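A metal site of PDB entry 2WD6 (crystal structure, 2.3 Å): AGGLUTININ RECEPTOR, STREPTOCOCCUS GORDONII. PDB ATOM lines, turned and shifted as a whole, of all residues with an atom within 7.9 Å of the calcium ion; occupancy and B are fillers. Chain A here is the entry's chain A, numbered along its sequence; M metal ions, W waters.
The calcium ion is bound by O of Ser 200 (2.3 Å), OG of Ser 200 (2.3 Å), OD1 of Asn 202 (2.3 Å), water W3 (2.4 Å), OE1 of Glu 216 (2.4 Å), water W2 (2.6 Å) and water W1 (2.7 Å). The calcium ion has seven donor atoms within binding distance.
Of the 18 residues printed, 3 come within 4 Å of the calcium ion.
The side-chain carboxylate (OD1) of Asp 262 lies close to the side-chain hydroxyl (OG) of Ser 200, at 2.7 Å. The backbone carbonyl oxygen (O) of Gly 272 sits at hydrogen-bond distance from the backbone NH (N) of Ser 200. OD2 of Asp 262 is in hydrogen-bond range of ND2 of Asn 202, at 2.8 Å.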
ATOM      1  N   TRP A 165      14.780  17.709 -16.327  1.00  0.00           N
ATOM      2  CA  TRP A 165      15.098  19.138 -16.201  1.00  0.00           C
ATOM      3  C   TRP A 165      15.556  19.353 -14.763  1.00  0.00           C
ATOM      4  O   TRP A 165      15.094  18.675 -13.828  1.00  0.00           O
ATOM      5  CB  TRP A 165      13.894  20.031 -16.505  1.00  0.00           C
ATOM      6  CG  TRP A 165      13.526  20.136 -17.950  1.00  0.00           C
ATOM      7  CD1 TRP A 165      12.869  19.193 -18.699  1.00  0.00           C
ATOM      8  CD2 TRP A 165      13.732  21.280 -18.843  1.00  0.00           C
ATOM      9  NE1 TRP A 165      12.683  19.661 -19.993  1.00  0.00           N
ATOM     10  CE2 TRP A 165      13.209  20.922 -20.112  1.00  0.00           C
ATOM     11  CE3 TRP A 165      14.344  22.549 -18.684  1.00  0.00           C
ATOM     12  CZ2 TRP A 165      13.245  21.811 -21.237  1.00  0.00           C
ATOM     13  CZ3 TRP A 165      14.374  23.462 -19.837  1.00  0.00           C
ATOM     14  CH2 TRP A 165      13.833  23.057 -21.093  1.00  0.00           C
ATOM     15  N   SER A 199      24.336  16.246 -25.448  1.00  0.00           N
ATOM     16  CA  SER A 199      23.948  17.180 -26.466  1.00  0.00           C
ATOM     17  C   SER A 199      23.512  18.457 -25.842  1.00  0.00           C
ATOM     18  O   SER A 199      23.309  18.504 -24.634  1.00  0.00           O
ATOM     19  CB  SER A 199      22.753  16.605 -27.265  1.00  0.00           C
ATOM     20  OG  SER A 199      21.719  16.382 -26.343  1.00  0.00           O
ATOM     21  N   SER A 200      23.282  19.482 -26.683  1.00  0.00           N
ATOM     22  CA  SER A 200      22.637  20.709 -26.214  1.00  0.00           C
ATOM     23  C   SER A 200      23.342  21.297 -24.962  1.00  0.00           C
ATOM     24  O   SER A 200      22.692  21.748 -23.985  1.00  0.00           O
ATOM     25  CB  SER A 200      21.141  20.451 -25.930  1.00  0.00           C
ATOM     26  OG  SER A 200      20.514  21.687 -25.574  1.00  0.00           O
ATOM     27  N   LEU A 201      24.672  21.329 -25.003  1.00  0.00           N
ATOM     28  CA  LEU A 201      25.422  21.895 -23.899  1.00  0.00           C
ATOM     29  C   LEU A 201      25.662  23.376 -24.205  1.00  0.00           C
ATOM     30  O   LEU A 201      26.721  23.795 -24.702  1.00  0.00           O
ATOM     31  CB  LEU A 201      26.736  21.126 -23.717  1.00  0.00           C
ATOM     32  CG  LEU A 201      26.562  19.657 -23.310  1.00  0.00           C
ATOM     33  CD1 LEU A 201      27.909  18.951 -23.386  1.00  0.00           C
ATOM     34  CD2 LEU A 201      25.962  19.550 -21.873  1.00  0.00           C
ATOM     35  N   ASN A 202      24.629  24.164 -23.958  1.00  0.00           N
ATOM     36  CA  ASN A 202      24.690  25.575 -24.241  1.00  0.00           C
ATOM     37  C   ASN A 202      25.668  26.351 -23.359  1.00  0.00           C
ATOM     38  O   ASN A 202      25.784  26.110 -22.149  1.00  0.00           O
ATOM     39  CB  ASN A 202      23.314  26.250 -24.180  1.00  0.00           C
ATOM     40  CG  ASN A 202      22.239  25.461 -24.880  1.00  0.00           C
ATOM     41  OD1 ASN A 202      21.779  24.519 -24.323  1.00  0.00           O
ATOM     42  ND2 ASN A 202      21.789  25.878 -26.067  1.00  0.00           N
ATOM     43  N   ARG A 203      26.336  27.280 -24.026  1.00  0.00           N
ATOM     44  CA  ARG A 203      27.043  28.367 -23.349  1.00  0.00           C
ATOM     45  C   ARG A 203      26.692  29.701 -23.996  1.00  0.00           C
ATOM     46  O   ARG A 203      26.700  29.796 -25.210  1.00  0.00           O
ATOM     47  CB  ARG A 203      28.552  28.163 -23.325  1.00  0.00           C
ATOM     48  CG  ARG A 203      29.201  29.257 -22.507  1.00  0.00           C
ATOM     49  CD  ARG A 203      30.703  29.035 -22.272  1.00  0.00           C
ATOM     50  NE  ARG A 203      31.194  30.058 -21.353  1.00  0.00           N
ATOM     51  CZ  ARG A 203      32.355  29.954 -20.715  1.00  0.00           C
ATOM     52  NH1 ARG A 203      33.099  28.881 -20.929  1.00  0.00           N
ATOM     53  NH2 ARG A 203      32.758  30.929 -19.877  1.00  0.00           N
ATOM     54  N   ASN A 205      23.730  31.379 -23.576  1.00  0.00           N
ATOM     55  CA  ASN A 205      22.311  31.505 -23.842  1.00  0.00           C
ATOM     56  C   ASN A 205      21.528  31.931 -22.585  1.00  0.00           C
ATOM     57  O   ASN A 205      20.348  31.587 -22.441  1.00  0.00           O
ATOM     58  CB  ASN A 205      21.781  30.175 -24.313  1.00  0.00           C
ATOM     59  CG  ASN A 205      21.820  29.129 -23.207  1.00  0.00           C
ATOM     60  OD1 ASN A 205      22.751  29.117 -22.364  1.00  0.00           O
ATOM     61  ND2 ASN A 205      20.784  28.268 -23.152  1.00  0.00           N
ATOM     62  N   GLU A 216      26.059  25.258 -19.595  1.00  0.00           N
ATOM     63  CA  GLU A 216      25.662  23.862 -19.310  1.00  0.00           C
ATOM     64  C   GLU A 216      26.826  22.925 -19.568  1.00  0.00           C
ATOM     65  O   GLU A 216      27.550  23.039 -20.578  1.00  0.00           O
ATOM     66  CB  GLU A 216      24.463  23.430 -20.132  1.00  0.00           C
ATOM     67  CG  GLU A 216      23.204  24.226 -19.746  1.00  0.00           C
ATOM     68  CD  GLU A 216      22.076  24.088 -20.782  1.00  0.00           C
ATOM     69  OE1 GLU A 216      22.045  23.033 -21.468  1.00  0.00           O
ATOM     70  OE2 GLU A 216      21.208  25.021 -20.895  1.00  0.00           O
ATOM     71  N   THR A 258      22.053  30.042 -31.292  1.00  0.00           N
ATOM     72  CA  THR A 258      21.401  28.904 -30.654  1.00  0.00           C
ATOM     73  C   THR A 258      20.279  28.303 -31.532  1.00  0.00           C
ATOM     74  O   THR A 258      20.259  27.105 -31.777  1.00  0.00           O
ATOM     75  CB  THR A 258      20.863  29.294 -29.296  1.00  0.00           C
ATOM     76  OG1 THR A 258      21.922  29.871 -28.527  1.00  0.00           O
ATOM     77  CG2 THR A 258      20.254  28.056 -28.498  1.00  0.00           C
ATOM     78  N   TRP A 261      21.077  25.715 -34.409  1.00  0.00           N
ATOM     79  CA  TRP A 261      21.661  24.393 -34.168  1.00  0.00           C
ATOM     80  C   TRP A 261      21.000  23.635 -33.027  1.00  0.00           C
ATOM     81  O   TRP A 261      21.077  22.396 -33.010  1.00  0.00           O
ATOM     82  CB  TRP A 261      23.200  24.492 -33.948  1.00  0.00           C
ATOM     83  CG  TRP A 261      23.593  25.137 -32.628  1.00  0.00           C
ATOM     84  CD1 TRP A 261      23.989  26.436 -32.443  1.00  0.00           C
ATOM     85  CD2 TRP A 261      23.625  24.514 -31.314  1.00  0.00           C
ATOM     86  NE1 TRP A 261      24.205  26.676 -31.113  1.00  0.00           N
ATOM     87  CE2 TRP A 261      24.029  25.528 -30.390  1.00  0.00           C
ATOM     88  CE3 TRP A 261      23.372  23.192 -30.832  1.00  0.00           C
ATOM     89  CZ2 TRP A 261      24.197  25.267 -28.982  1.00  0.00           C
ATOM     90  CZ3 TRP A 261      23.497  22.937 -29.410  1.00  0.00           C
ATOM     91  CH2 TRP A 261      23.912  23.980 -28.513  1.00  0.00           C
ATOM     92  N   ASP A 262      20.406  24.323 -32.061  1.00  0.00           N
ATOM     93  CA  ASP A 262      20.042  23.624 -30.813  1.00  0.00           C
ATOM     94  C   ASP A 262      18.631  23.045 -30.824  1.00  0.00           C
ATOM     95  O   ASP A 262      17.756  23.467 -30.065  1.00  0.00           O
ATOM     96  CB  ASP A 262      20.314  24.461 -29.573  1.00  0.00           C
ATOM     97  CG  ASP A 262      20.041  23.722 -28.255  1.00  0.00           C
ATOM     98  OD1 ASP A 262      20.106  22.452 -28.141  1.00  0.00           O
ATOM     99  OD2 ASP A 262      19.745  24.452 -27.261  1.00  0.00           O
ATOM    100  N   GLY A 272      26.775  21.609 -30.598  1.00  0.00           N
ATOM    101  CA  GLY A 272      26.666  21.682 -29.139  1.00  0.00           C
ATOM    102  C   GLY A 272      26.749  20.325 -28.454  1.00  0.00           C
ATOM    103  O   GLY A 272      26.262  20.156 -27.344  1.00  0.00           O
ATOM    104  N   SER A 292      21.884  29.383 -15.467  1.00  0.00           N
ATOM    105  CA  SER A 292      20.943  28.891 -16.507  1.00  0.00           C
ATOM    106  C   SER A 292      19.481  29.006 -16.187  1.00  0.00           C
ATOM    107  O   SER A 292      18.688  29.096 -17.124  1.00  0.00           O
ATOM    108  CB  SER A 292      21.242  27.463 -16.884  1.00  0.00           C
ATOM    109  OG  SER A 292      22.486  27.374 -17.532  1.00  0.00           O
ATOM    110  N   ASN A 294      16.735  27.197 -15.851  1.00  0.00           N
ATOM    111  CA  ASN A 294      16.192  25.833 -16.154  1.00  0.00           C
ATOM    112  C   ASN A 294      17.164  25.120 -17.050  1.00  0.00           C
ATOM    113  O   ASN A 294      17.685  25.700 -18.010  1.00  0.00           O
ATOM    114  CB  ASN A 294      14.890  25.871 -16.945  1.00  0.00           C
ATOM    115  CG  ASN A 294      13.776  26.552 -16.229  1.00  0.00           C
ATOM    116  OD1 ASN A 294      13.864  26.796 -15.036  1.00  0.00           O
ATOM    117  ND2 ASN A 294      12.693  26.833 -16.951  1.00  0.00           N
ATOM    118  N   ILE A 295      17.413  23.855 -16.763  1.00  0.00           N
ATOM    119  CA  ILE A 295      18.373  23.111 -17.577  1.00  0.00           C
ATOM    120  C   ILE A 295      17.749  21.773 -17.979  1.00  0.00           C
ATOM    121  O   ILE A 295      17.205  21.100 -17.137  1.00  0.00           O
ATOM    122  CB  ILE A 295      19.709  22.912 -16.855  1.00  0.00           C
ATOM    123  CG1 ILE A 295      20.301  24.284 -16.451  1.00  0.00           C
ATOM    124  CG2 ILE A 295      20.669  22.225 -17.743  1.00  0.00           C
ATOM    125  CD1 ILE A 295      20.048  24.683 -14.968  1.00  0.00           C
ATOM    126  N   TRP A 296      17.760  21.494 -19.278  1.00  0.00           N
ATOM    127  CA  TRP A 296      17.312  20.253 -19.816  1.00  0.00           C
ATOM    128  C   TRP A 296      18.540  19.362 -19.986  1.00  0.00           C
ATOM    129  O   TRP A 296      19.523  19.785 -20.597  1.00  0.00           O
ATOM    130  CB  TRP A 296      16.653  20.450 -21.185  1.00  0.00           C
ATOM    131  CG  TRP A 296      16.144  19.116 -21.748  1.00  0.00           C
ATOM    132  CD1 TRP A 296      15.733  18.029 -21.026  1.00  0.00           C
ATOM    133  CD2 TRP A 296      15.987  18.757 -23.124  1.00  0.00           C
ATOM    134  NE1 TRP A 296      15.346  17.036 -21.843  1.00  0.00           N
ATOM    135  CE2 TRP A 296      15.471  17.444 -23.148  1.00  0.00           C
ATOM    136  CE3 TRP A 296      16.209  19.425 -24.339  1.00  0.00           C
ATOM    137  CZ2 TRP A 296      15.168  16.758 -24.355  1.00  0.00           C
ATOM    138  CZ3 TRP A 296      15.909  18.748 -25.546  1.00  0.00           C
ATOM    139  CH2 TRP A 296      15.419  17.423 -25.528  1.00  0.00           C
ATOM    140  N   PHE A 297      18.491  18.170 -19.411  1.00  0.00           N
ATOM    141  CA  PHE A 297      19.570  17.212 -19.643  1.00  0.00           C
ATOM    142  C   PHE A 297      19.000  15.876 -20.094  1.00  0.00           C
ATOM    143  O   PHE A 297      18.428  15.130 -19.298  1.00  0.00           O
ATOM    144  CB  PHE A 297      20.423  17.042 -18.411  1.00  0.00           C
ATOM    145  CG  PHE A 297      21.758  16.382 -18.684  1.00  0.00           C
ATOM    146  CD1 PHE A 297      22.932  17.129 -18.628  1.00  0.00           C
ATOM    147  CD2 PHE A 297      21.844  15.012 -18.942  1.00  0.00           C
ATOM    148  CE1 PHE A 297      24.198  16.526 -18.829  1.00  0.00           C
ATOM    149  CE2 PHE A 297      23.048  14.404 -19.187  1.00  0.00           C
ATOM    150  CZ  PHE A 297      24.259  15.168 -19.129  1.00  0.00           C
ATOM    151  N   ALA A 298      19.152  15.605 -21.376  1.00  0.00           N
ATOM    152  CA  ALA A 298      18.665  14.383 -21.984  1.00  0.00           C
ATOM    153  C   ALA A 298      19.799  13.352 -22.056  1.00  0.00           C
ATOM    154  O   ALA A 298      20.890  13.662 -22.542  1.00  0.00           O
ATOM    155  CB  ALA A 298      18.114  14.678 -23.397  1.00  0.00           C
HETATM  156 CA    CA M   1      20.677  22.635 -23.453  1.00  0.00          CA
HETATM  157  O   HOH W   1      18.537  24.138 -24.250  1.00  0.00           O
HETATM  158  O   HOH W   2      18.835  23.631 -21.873  1.00  0.00           O
HETATM  159  O   HOH W   3      19.795  20.501 -22.829  1.00  0.00           O
